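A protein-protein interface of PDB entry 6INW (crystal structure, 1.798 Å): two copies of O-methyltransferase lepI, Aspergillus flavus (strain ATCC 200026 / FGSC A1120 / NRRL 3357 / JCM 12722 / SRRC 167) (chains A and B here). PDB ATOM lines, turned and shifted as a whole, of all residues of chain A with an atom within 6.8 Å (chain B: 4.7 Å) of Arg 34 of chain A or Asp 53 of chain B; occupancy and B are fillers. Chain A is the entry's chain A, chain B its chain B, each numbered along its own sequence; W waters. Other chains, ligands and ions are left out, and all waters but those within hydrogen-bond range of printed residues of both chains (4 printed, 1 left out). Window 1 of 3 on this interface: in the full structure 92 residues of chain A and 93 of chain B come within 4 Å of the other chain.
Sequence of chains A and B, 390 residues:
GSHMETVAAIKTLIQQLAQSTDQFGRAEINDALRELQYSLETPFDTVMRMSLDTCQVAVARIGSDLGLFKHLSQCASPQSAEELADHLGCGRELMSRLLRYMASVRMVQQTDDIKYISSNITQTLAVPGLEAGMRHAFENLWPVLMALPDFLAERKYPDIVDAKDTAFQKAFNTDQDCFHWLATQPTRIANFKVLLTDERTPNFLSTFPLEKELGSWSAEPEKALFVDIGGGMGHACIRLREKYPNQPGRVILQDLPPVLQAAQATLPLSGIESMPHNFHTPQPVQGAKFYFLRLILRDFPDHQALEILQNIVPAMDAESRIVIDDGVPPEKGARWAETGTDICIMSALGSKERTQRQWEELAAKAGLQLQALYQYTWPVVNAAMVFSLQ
The side-chain amide nitrogen (ND2) of Asn 30 of chain A lies within hydrogen-bond range of the backbone carbonyl oxygen (O) of Gln 37 of chain B (3.2 Å). The guanidinium group of Arg 34 of chain A sits close to the side-chain amide nitrogen of Gln 37 of chain B. The guanidinium group of Arg 34 of chain A lies within salt-bridge range of the side-chain carboxylate of Asp 53 of chain B (3.0 Å). The side-chain hydroxyl (OH) of Tyr 38 of chain A lies within hydrogen-bond range of the side-chain amide nitrogen (NE2) of Gln 56 of chain B (2.9 Å). NH1 of Arg 49 of chain A is in hydrogen-bond range of OE1 of Gln 56 of chain B, at 2.8 Å. The side-chain amide oxygen of Gln 56 of chain A sits at hydrogen-bond distance from the guanidinium group of Arg 49 of chain B, 2.9 Å away.
NE1 of Trp 336 of chain A lies within hydrogen-bond range of OD1 of Asp 31 of chain A, at 3.4 Å. The side-chain hydroxyl of Tyr 38 of chain A lies within hydrogen-bond range of the guanidinium group of Arg 34 of chain A, 3.2 Å away.
N of Gln 37 of chain B touches CD1 of Leu 33 of chain A, 3.97 Å away. CD of Arg 49 of chain B touches NH2 of Arg 34 of chain A, at 3.8 Å. Gln 37 of chain A touches Gln 37 of chain B (NE2 to OE1, 3.7 Å). Gln 56 of chain B touches Met 50 of chain A. Met 50 of chain A touches Val 57 of chain B. OG1 of Thr 54 of chain B touches CD1 of Leu 145 of chain A, at 3.3 Å. CD1 of Leu 145 of chain A touches SG of Cys 55 of chain B (3.6 Å). Met 48 of chain B touches Trp 336 of chain A (O to CZ3, 3.8 Å). Trp 336 of chain A touches Arg 49 of chain B (CH2 to CA, 3.7 Å). Trp 336 of chain A touches Leu 52 of chain B (CZ3 to CD1, 3.8 Å).
Of chain B, only Gln 37, Arg 49 and Asp 53 come within 4 Å of Arg 34 of chain A. Leu 36 of chain A touches none of the printed residues of chain B. Of the printed residues of chain B, Gln 37 of chain A touches Gln 37 (3.7 Å). Of the printed residues of chain B, Arg 49 of chain A touches Gln 56 (2.8 Å). Of the printed residues of chain B, Leu 145 of chain A touches Thr 54 (3.3 Å) and Cys 55 (3.6 Å). Of the printed residues of chain B, Trp 336 of chain A touches Met 48, Arg 49 and Leu 52. Ser 51 of chain B touches none of the printed residues of chain A. Asp 53 of chain B touches just one residue of chain A: Arg 34 (3.0 Å). The nearest residue of chain A that does not touch Asp 53 of chain B is Trp 336 of chain A (4.2 Å).
Hydrophobic or aromatic side chains of chain A that line the printed part of chain B: Leu 33, Tyr 38, Met 50, Leu 145 and Trp 336. Printed residues of chain B that touch a printed residue of chain A: Gln 37, Met 48, Arg 49, Met 50, Leu 52, Asp 53, Thr 54, Cys 55, Gln 56 and Val 57.
Gln 37 of chain B touches its own counterpart, Gln 37 of chain A. Arg 49 of chain A touches Gln 56 of chain B, and with the chains exchanged Gln 56 of chain A touches Arg 49 of chain B. Met 50 of chain A touches Gln 56 of chain B, and with the chains exchanged Gln 56 of chain A touches Met 50 of chain B.
Water W3 lies within hydrogen-bond range of the side-chain amide nitrogen of Gln 37 of chain B (2.7 Å), the guanidinium group of Arg 34 of chain A (2.7 Å) and the side-chain carboxylate of Asp 53 of chain B (2.9 Å). Water W4 lies within hydrogen-bond range of the side-chain amide oxygen of Gln 56 of chain A and the guanidinium group of Arg 49 of chain B. Water W1 bridges the side-chain amide oxygen (OE1) of Gln 56 of chain B (2.9 Å) and the guanidinium group (NH2) of Arg 49 of chain A (3.0 Å). Water W2 bridges NE2 of Gln 37 of chain A (3.0 Å) and OE1 of Gln 37 of chain B (3.2 Å).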
ATOM      1  N   ILE A  29     -24.345  -7.028  19.772  1.00  0.00           N
ATOM      2  CA  ILE A  29     -23.153  -7.857  19.612  1.00  0.00           C
ATOM      3  C   ILE A  29     -23.306  -9.166  20.380  1.00  0.00           C
ATOM      4  O   ILE A  29     -22.951 -10.237  19.877  1.00  0.00           O
ATOM      5  CB  ILE A  29     -21.895  -7.088  20.056  1.00  0.00           C
ATOM      6  CG1 ILE A  29     -21.538  -6.005  19.037  1.00  0.00           C
ATOM      7  CG2 ILE A  29     -20.715  -8.041  20.245  1.00  0.00           C
ATOM      8  CD1 ILE A  29     -20.416  -5.088  19.495  1.00  0.00           C
ATOM      9  N   ASN A  30     -23.835  -9.103  21.606  1.00  0.00           N
ATOM     10  CA  ASN A  30     -23.998 -10.317  22.405  1.00  0.00           C
ATOM     11  C   ASN A  30     -24.971 -11.290  21.748  1.00  0.00           C
ATOM     12  O   ASN A  30     -24.729 -12.507  21.722  1.00  0.00           O
ATOM     13  CB  ASN A  30     -24.472  -9.963  23.814  1.00  0.00           C
ATOM     14  CG  ASN A  30     -23.370 -10.093  24.844  1.00  0.00           C
ATOM     15  OD1 ASN A  30     -22.189  -9.980  24.519  1.00  0.00           O
ATOM     16  ND2 ASN A  30     -23.751 -10.337  26.091  1.00  0.00           N
ATOM     17  N   ASP A  31     -26.084 -10.773  21.221  1.00  0.00           N
ATOM     18  CA  ASP A  31     -27.013 -11.641  20.500  1.00  0.00           C
ATOM     19  C   ASP A  31     -26.345 -12.267  19.279  1.00  0.00           C
ATOM     20  O   ASP A  31     -26.584 -13.441  18.962  1.00  0.00           O
ATOM     21  CB  ASP A  31     -28.261 -10.856  20.089  1.00  0.00           C
ATOM     22  CG  ASP A  31     -29.244 -10.681  21.235  1.00  0.00           C
ATOM     23  OD1 ASP A  31     -28.960 -11.179  22.346  1.00  0.00           O
ATOM     24  OD2 ASP A  31     -30.300 -10.044  21.028  1.00  0.00           O
ATOM     25  N   ALA A  32     -25.497 -11.500  18.586  1.00  0.00           N
ATOM     26  CA  ALA A  32     -24.785 -12.046  17.434  1.00  0.00           C
ATOM     27  C   ALA A  32     -23.826 -13.154  17.849  1.00  0.00           C
ATOM     28  O   ALA A  32     -23.695 -14.166  17.151  1.00  0.00           O
ATOM     29  CB  ALA A  32     -24.034 -10.935  16.703  1.00  0.00           C
ATOM     30  N   LEU A  33     -23.134 -12.974  18.975  1.00  0.00           N
ATOM     31  CA  LEU A  33     -22.229 -14.011  19.460  1.00  0.00           C
ATOM     32  C   LEU A  33     -22.994 -15.285  19.781  1.00  0.00           C
ATOM     33  O   LEU A  33     -22.534 -16.393  19.475  1.00  0.00           O
ATOM     34  CB  LEU A  33     -21.470 -13.527  20.698  1.00  0.00           C
ATOM     35  CG  LEU A  33     -20.553 -12.313  20.531  1.00  0.00           C
ATOM     36  CD1 LEU A  33     -19.995 -11.872  21.877  1.00  0.00           C
ATOM     37  CD2 LEU A  33     -19.430 -12.605  19.549  1.00  0.00           C
ATOM     38  N   ARG A  34     -24.167 -15.145  20.400  1.00  0.00           N
ATOM     39  CA  ARG A  34     -24.989 -16.317  20.692  1.00  0.00           C
ATOM     40  C   ARG A  34     -25.420 -17.022  19.408  1.00  0.00           C
ATOM     41  O   ARG A  34     -25.348 -18.256  19.302  1.00  0.00           O
ATOM     42  CB  ARG A  34     -26.206 -15.903  21.522  1.00  0.00           C
ATOM     43  CG  ARG A  34     -27.118 -17.058  21.901  1.00  0.00           C
ATOM     44  CD  ARG A  34     -28.367 -16.559  22.601  1.00  0.00           C
ATOM     45  NE  ARG A  34     -28.095 -16.117  23.966  1.00  0.00           N
ATOM     46  CZ  ARG A  34     -28.641 -16.662  25.049  1.00  0.00           C
ATOM     47  NH1 ARG A  34     -29.493 -17.671  24.928  1.00  0.00           N
ATOM     48  NH2 ARG A  34     -28.339 -16.197  26.252  1.00  0.00           N
ATOM     49  N   GLU A  35     -25.892 -16.250  18.422  1.00  0.00           N
ATOM     50  CA  GLU A  35     -26.308 -16.842  17.154  1.00  0.00           C
ATOM     51  C   GLU A  35     -25.146 -17.553  16.469  1.00  0.00           C
ATOM     52  O   GLU A  35     -25.317 -18.638  15.897  1.00  0.00           O
ATOM     53  CB  GLU A  35     -26.893 -15.768  16.237  1.00  0.00           C
ATOM     54  CG  GLU A  35     -27.325 -16.299  14.878  1.00  0.00           C
ATOM     55  CD  GLU A  35     -27.781 -15.199  13.938  1.00  0.00           C
ATOM     56  OE1 GLU A  35     -28.851 -14.606  14.194  1.00  0.00           O
ATOM     57  OE2 GLU A  35     -27.072 -14.931  12.943  1.00  0.00           O
ATOM     58  N   LEU A  36     -23.954 -16.956  16.522  1.00  0.00           N
ATOM     59  CA  LEU A  36     -22.777 -17.588  15.937  1.00  0.00           C
ATOM     60  C   LEU A  36     -22.450 -18.893  16.643  1.00  0.00           C
ATOM     61  O   LEU A  36     -22.134 -19.897  15.994  1.00  0.00           O
ATOM     62  CB  LEU A  36     -21.582 -16.637  16.009  1.00  0.00           C
ATOM     63  CG  LEU A  36     -21.510 -15.586  14.904  1.00  0.00           C
ATOM     64  CD1 LEU A  36     -20.483 -14.506  15.245  1.00  0.00           C
ATOM     65  CD2 LEU A  36     -21.182 -16.254  13.581  1.00  0.00           C
ATOM     66  N   GLN A  37     -22.511 -18.891  17.976  1.00  0.00           N
ATOM     67  CA  GLN A  37     -22.248 -20.108  18.733  1.00  0.00           C
ATOM     68  C   GLN A  37     -23.214 -21.218  18.333  1.00  0.00           C
ATOM     69  O   GLN A  37     -22.798 -22.348  18.048  1.00  0.00           O
ATOM     70  CB  GLN A  37     -22.339 -19.803  20.228  1.00  0.00           C
ATOM     71  CG  GLN A  37     -22.236 -21.006  21.135  1.00  0.00           C
ATOM     72  CD  GLN A  37     -22.559 -20.663  22.576  1.00  0.00           C
ATOM     73  OE1 GLN A  37     -22.979 -21.524  23.349  1.00  0.00           O
ATOM     74  NE2 GLN A  37     -22.363 -19.398  22.946  1.00  0.00           N
ATOM     75  N   TYR A  38     -24.512 -20.900  18.268  1.00  0.00           N
ATOM     76  CA  TYR A  38     -25.495 -21.917  17.892  1.00  0.00           C
ATOM     77  C   TYR A  38     -25.266 -22.411  16.468  1.00  0.00           C
ATOM     78  O   TYR A  38     -25.431 -23.603  16.183  1.00  0.00           O
ATOM     79  CB  TYR A  38     -26.918 -21.374  18.030  1.00  0.00           C
ATOM     80  CG  TYR A  38     -27.353 -21.086  19.449  1.00  0.00           C
ATOM     81  CD1 TYR A  38     -26.537 -21.393  20.534  1.00  0.00           C
ATOM     82  CD2 TYR A  38     -28.583 -20.495  19.703  1.00  0.00           C
ATOM     83  CE1 TYR A  38     -26.940 -21.120  21.833  1.00  0.00           C
ATOM     84  CE2 TYR A  38     -28.996 -20.221  20.994  1.00  0.00           C
ATOM     85  CZ  TYR A  38     -28.174 -20.534  22.055  1.00  0.00           C
ATOM     86  OH  TYR A  38     -28.595 -20.255  23.336  1.00  0.00           O
ATOM     87  N   SER A  39     -24.898 -21.509  15.556  1.00  0.00           N
ATOM     88  CA  SER A  39     -24.722 -21.917  14.167  1.00  0.00           C
ATOM     89  C   SER A  39     -23.463 -22.754  13.976  1.00  0.00           C
ATOM     90  O   SER A  39     -23.423 -23.605  13.082  1.00  0.00           O
ATOM     91  CB  SER A  39     -24.688 -20.688  13.255  1.00  0.00           C
ATOM     92  OG  SER A  39     -23.387 -20.132  13.202  1.00  0.00           O
ATOM     93  N   ARG A  49     -24.720 -28.750  25.214  1.00  0.00           N
ATOM     94  CA  ARG A  49     -25.069 -27.426  25.711  1.00  0.00           C
ATOM     95  C   ARG A  49     -26.431 -27.448  26.388  1.00  0.00           C
ATOM     96  O   ARG A  49     -26.597 -26.921  27.495  1.00  0.00           O
ATOM     97  CB  ARG A  49     -25.047 -26.417  24.561  1.00  0.00           C
ATOM     98  CG  ARG A  49     -25.881 -25.170  24.804  1.00  0.00           C
ATOM     99  CD  ARG A  49     -25.662 -24.132  23.707  1.00  0.00           C
ATOM    100  NE  ARG A  49     -26.355 -24.466  22.465  1.00  0.00           N
ATOM    101  CZ  ARG A  49     -27.670 -24.368  22.291  1.00  0.00           C
ATOM    102  NH1 ARG A  49     -28.447 -23.950  23.282  1.00  0.00           N
ATOM    103  NH2 ARG A  49     -28.211 -24.685  21.123  1.00  0.00           N
ATOM    104  N   MET A  50     -27.416 -28.073  25.747  1.00  0.00           N
ATOM    105  CA  MET A  50     -28.744 -28.149  26.344  1.00  0.00           C
ATOM    106  C   MET A  50     -28.759 -28.992  27.622  1.00  0.00           C
ATOM    107  O   MET A  50     -29.532 -28.727  28.539  1.00  0.00           O
ATOM    108  CB  MET A  50     -29.745 -28.699  25.330  1.00  0.00           C
ATOM    109  CG  MET A  50     -30.011 -27.736  24.194  1.00  0.00           C
ATOM    110  SD  MET A  50     -31.310 -28.426  22.929  1.00  0.00           S
ATOM    111  CE  MET A  50     -31.257 -26.977  21.626  1.00  0.00           C
ATOM    112  N   ASP A  53     -26.145 -26.530  30.358  1.00  0.00           N
ATOM    113  CA  ASP A  53     -26.391 -25.143  30.741  1.00  0.00           C
ATOM    114  C   ASP A  53     -27.406 -25.038  31.874  1.00  0.00           C
ATOM    115  O   ASP A  53     -27.458 -24.006  32.553  1.00  0.00           O
ATOM    116  CB  ASP A  53     -26.832 -24.334  29.517  1.00  0.00           C
ATOM    117  CG  ASP A  53     -25.657 -23.973  28.604  1.00  0.00           C
ATOM    118  OD1 ASP A  53     -24.513 -24.373  28.906  1.00  0.00           O
ATOM    119  OD2 ASP A  53     -25.876 -23.292  27.580  1.00  0.00           O
ATOM    120  N   THR A  54     -28.193 -26.094  32.101  1.00  0.00           N
ATOM    121  CA  THR A  54     -29.110 -26.141  33.238  1.00  0.00           C
ATOM    122  C   THR A  54     -28.362 -26.118  34.570  1.00  0.00           C
ATOM    123  O   THR A  54     -28.916 -25.682  35.588  1.00  0.00           O
ATOM    124  CB  THR A  54     -29.974 -27.406  33.140  1.00  0.00           C
ATOM    125  OG1 THR A  54     -30.641 -27.439  31.873  1.00  0.00           O
ATOM    126  CG2 THR A  54     -31.015 -27.458  34.247  1.00  0.00           C
ATOM    127  N   GLN A  56     -26.128 -24.151  35.513  1.00  0.00           N
ATOM    128  CA  GLN A  56     -25.754 -22.813  35.956  1.00  0.00           C
ATOM    129  C   GLN A  56     -26.696 -22.296  37.036  1.00  0.00           C
ATOM    130  O   GLN A  56     -26.243 -21.743  38.043  1.00  0.00           O
ATOM    131  CB  GLN A  56     -25.718 -21.855  34.765  1.00  0.00           C
ATOM    132  CG  GLN A  56     -24.640 -22.193  33.747  1.00  0.00           C
ATOM    133  CD  GLN A  56     -24.211 -20.997  32.920  1.00  0.00           C
ATOM    134  OE1 GLN A  56     -24.199 -19.864  33.403  1.00  0.00           O
ATOM    135  NE2 GLN A  56     -23.853 -21.246  31.665  1.00  0.00           N
ATOM    136  N   LEU A 145     -41.673 -24.763  34.158  1.00  0.00           N
ATOM    137  CA  LEU A 145     -41.128 -25.226  32.886  1.00  0.00           C
ATOM    138  C   LEU A 145     -40.971 -26.742  32.861  1.00  0.00           C
ATOM    139  O   LEU A 145     -41.143 -27.361  31.805  1.00  0.00           O
ATOM    140  CB  LEU A 145     -39.790 -24.547  32.602  1.00  0.00           C
ATOM    141  CG  LEU A 145     -39.899 -23.041  32.359  1.00  0.00           C
ATOM    142  CD1 LEU A 145     -38.521 -22.408  32.223  1.00  0.00           C
ATOM    143  CD2 LEU A 145     -40.755 -22.765  31.128  1.00  0.00           C
ATOM    144  N   TRP A 336     -34.648 -13.856  21.930  1.00  0.00           N
ATOM    145  CA  TRP A 336     -34.871 -14.881  22.949  1.00  0.00           C
ATOM    146  C   TRP A 336     -35.353 -14.282  24.266  1.00  0.00           C
ATOM    147  O   TRP A 336     -36.101 -14.933  25.001  1.00  0.00           O
ATOM    148  CB  TRP A 336     -33.595 -15.703  23.172  1.00  0.00           C
ATOM    149  CG  TRP A 336     -32.451 -14.923  23.760  1.00  0.00           C
ATOM    150  CD1 TRP A 336     -31.452 -14.294  23.077  1.00  0.00           C
ATOM    151  CD2 TRP A 336     -32.198 -14.682  25.151  1.00  0.00           C
ATOM    152  NE1 TRP A 336     -30.594 -13.677  23.954  1.00  0.00           N
ATOM    153  CE2 TRP A 336     -31.028 -13.902  25.233  1.00  0.00           C
ATOM    154  CE3 TRP A 336     -32.847 -15.053  26.336  1.00  0.00           C
ATOM    155  CZ2 TRP A 336     -30.495 -13.481  26.452  1.00  0.00           C
ATOM    156  CZ3 TRP A 336     -32.317 -14.635  27.543  1.00  0.00           C
ATOM    157  CH2 TRP A 336     -31.152 -13.859  27.592  1.00  0.00           C
ATOM    158  N   GLN B  37     -19.453 -13.525  25.445  1.00  0.00           N
ATOM    159  CA  GLN B  37     -20.838 -13.223  25.786  1.00  0.00           C
ATOM    160  C   GLN B  37     -20.997 -13.023  27.289  1.00  0.00           C
ATOM    161  O   GLN B  37     -21.621 -12.051  27.736  1.00  0.00           O
ATOM    162  CB  GLN B  37     -21.742 -14.343  25.271  1.00  0.00           C
ATOM    163  CG  GLN B  37     -23.190 -14.240  25.676  1.00  0.00           C
ATOM    164  CD  GLN B  37     -23.956 -15.503  25.342  1.00  0.00           C
ATOM    165  OE1 GLN B  37     -23.646 -16.188  24.362  1.00  0.00           O
ATOM    166  NE2 GLN B  37     -24.955 -15.825  26.157  1.00  0.00           N
ATOM    167  N   MET B  48     -31.278 -12.650  33.363  1.00  0.00           N
ATOM    168  CA  MET B  48     -32.235 -13.010  32.322  1.00  0.00           C
ATOM    169  C   MET B  48     -31.823 -14.294  31.600  1.00  0.00           C
ATOM    170  O   MET B  48     -32.650 -15.174  31.337  1.00  0.00           O
ATOM    171  CB  MET B  48     -32.372 -11.852  31.329  1.00  0.00           C
ATOM    172  CG  MET B  48     -33.535 -11.957  30.352  1.00  0.00           C
ATOM    173  SD  MET B  48     -35.298 -11.993  31.180  1.00  0.00           S
ATOM    174  CE  MET B  48     -35.008 -10.843  32.717  1.00  0.00           C
ATOM    175  N   ARG B  49     -30.530 -14.389  31.284  1.00  0.00           N
ATOM    176  CA  ARG B  49     -29.999 -15.578  30.633  1.00  0.00           C
ATOM    177  C   ARG B  49     -30.202 -16.808  31.505  1.00  0.00           C
ATOM    178  O   ARG B  49     -30.699 -17.841  31.041  1.00  0.00           O
ATOM    179  CB  ARG B  49     -28.517 -15.367  30.319  1.00  0.00           C
ATOM    180  CG  ARG B  49     -27.731 -16.629  30.057  1.00  0.00           C
ATOM    181  CD  ARG B  49     -26.341 -16.297  29.531  1.00  0.00           C
ATOM    182  NE  ARG B  49     -25.453 -15.775  30.572  1.00  0.00           N
ATOM    183  CZ  ARG B  49     -24.905 -16.519  31.530  1.00  0.00           C
ATOM    184  NH1 ARG B  49     -25.158 -17.820  31.588  1.00  0.00           N
ATOM    185  NH2 ARG B  49     -24.102 -15.965  32.429  1.00  0.00           N
ATOM    186  N   MET B  50     -29.830 -16.712  32.776  1.00  0.00           N
ATOM    187  CA  MET B  50     -30.015 -17.840  33.680  1.00  0.00           C
ATOM    188  C   MET B  50     -31.490 -18.204  33.825  1.00  0.00           C
ATOM    189  O   MET B  50     -31.840 -19.374  33.940  1.00  0.00           O
ATOM    190  CB  MET B  50     -29.405 -17.534  35.044  1.00  0.00           C
ATOM    191  CG  MET B  50     -27.903 -17.689  35.055  1.00  0.00           C
ATOM    192  SD  MET B  50     -27.103 -17.138  36.730  1.00  0.00           S
ATOM    193  CE  MET B  50     -25.238 -17.191  36.171  1.00  0.00           C
ATOM    194  N   SER B  51     -32.359 -17.192  33.793  1.00  0.00           N
ATOM    195  CA  SER B  51     -33.785 -17.442  33.949  1.00  0.00           C
ATOM    196  C   SER B  51     -34.367 -18.148  32.731  1.00  0.00           C
ATOM    197  O   SER B  51     -35.218 -19.034  32.871  1.00  0.00           O
ATOM    198  CB  SER B  51     -34.525 -16.125  34.198  1.00  0.00           C
ATOM    199  OG  SER B  51     -34.096 -15.506  35.398  1.00  0.00           O
ATOM    200  N   LEU B  52     -33.928 -17.771  31.526  1.00  0.00           N
ATOM    201  CA  LEU B  52     -34.631 -18.170  30.312  1.00  0.00           C
ATOM    202  C   LEU B  52     -33.962 -19.265  29.494  1.00  0.00           C
ATOM    203  O   LEU B  52     -34.654 -19.919  28.707  1.00  0.00           O
ATOM    204  CB  LEU B  52     -34.851 -16.953  29.400  1.00  0.00           C
ATOM    205  CG  LEU B  52     -35.693 -15.812  29.976  1.00  0.00           C
ATOM    206  CD1 LEU B  52     -35.892 -14.733  28.928  1.00  0.00           C
ATOM    207  CD2 LEU B  52     -37.036 -16.323  30.489  1.00  0.00           C
ATOM    208  N   ASP B  53     -32.649 -19.482  29.624  1.00  0.00           N
ATOM    209  CA  ASP B  53     -32.015 -20.510  28.801  1.00  0.00           C
ATOM    210  C   ASP B  53     -32.507 -21.909  29.145  1.00  0.00           C
ATOM    211  O   ASP B  53     -32.412 -22.812  28.307  1.00  0.00           O
ATOM    212  CB  ASP B  53     -30.491 -20.431  28.940  1.00  0.00           C
ATOM    213  CG  ASP B  53     -29.888 -19.281  28.139  1.00  0.00           C
ATOM    214  OD1 ASP B  53     -30.657 -18.517  27.518  1.00  0.00           O
ATOM    215  OD2 ASP B  53     -28.646 -19.133  28.133  1.00  0.00           O
ATOM    216  N   THR B  54     -33.052 -22.100  30.348  1.00  0.00           N
ATOM    217  CA  THR B  54     -33.659 -23.369  30.733  1.00  0.00           C
ATOM    218  C   THR B  54     -34.909 -23.686  29.918  1.00  0.00           C
ATOM    219  O   THR B  54     -35.299 -24.857  29.832  1.00  0.00           O
ATOM    220  CB  THR B  54     -33.973 -23.345  32.228  1.00  0.00           C
ATOM    221  OG1 THR B  54     -35.278 -22.793  32.439  1.00  0.00           O
ATOM    222  CG2 THR B  54     -32.944 -22.476  32.944  1.00  0.00           C
ATOM    223  N   CYS B  55     -35.552 -22.667  29.338  1.00  0.00           N
ATOM    224  CA  CYS B  55     -36.720 -22.899  28.495  1.00  0.00           C
ATOM    225  C   CYS B  55     -36.376 -23.772  27.295  1.00  0.00           C
ATOM    226  O   CYS B  55     -37.258 -24.437  26.741  1.00  0.00           O
ATOM    227  CB  CYS B  55     -37.290 -21.567  28.000  1.00  0.00           C
ATOM    228  SG  CYS B  55     -38.516 -20.791  29.056  1.00  0.00           S
ATOM    229  N   GLN B  56     -35.110 -23.760  26.867  1.00  0.00           N
ATOM    230  CA  GLN B  56     -34.733 -24.474  25.651  1.00  0.00           C
ATOM    231  C   GLN B  56     -34.984 -25.968  25.787  1.00  0.00           C
ATOM    232  O   GLN B  56     -35.509 -26.597  24.864  1.00  0.00           O
ATOM    233  CB  GLN B  56     -33.266 -24.212  25.312  1.00  0.00           C
ATOM    234  CG  GLN B  56     -32.956 -22.763  24.987  1.00  0.00           C
ATOM    235  CD  GLN B  56     -31.661 -22.609  24.221  1.00  0.00           C
ATOM    236  OE1 GLN B  56     -31.252 -23.506  23.485  1.00  0.00           O
ATOM    237  NE2 GLN B  56     -31.003 -21.468  24.396  1.00  0.00           N
ATOM    238  N   VAL B  57     -34.620 -26.555  26.930  1.00  0.00           N
ATOM    239  CA  VAL B  57     -34.797 -27.998  27.099  1.00  0.00           C
ATOM    240  C   VAL B  57     -36.279 -28.361  27.142  1.00  0.00           C
ATOM    241  O   VAL B  57     -36.709 -29.347  26.530  1.00  0.00           O
ATOM    242  CB  VAL B  57     -34.066 -28.485  28.362  1.00  0.00           C
ATOM    243  CG1 VAL B  57     -34.214 -29.995  28.502  1.00  0.00           C
ATOM    244  CG2 VAL B  57     -32.606 -28.096  28.307  1.00  0.00           C
HETATM  245  O   HOH W   1     -31.018 -23.841  20.609  1.00  0.00           O
HETATM  246  O   HOH W   2     -24.493 -19.160  25.076  1.00  0.00           O
HETATM  247  O   HOH W   3     -26.396 -18.077  26.660  1.00  0.00           O
HETATM  248  O   HOH W   4     -22.494 -17.846  34.137  1.00  0.00           O
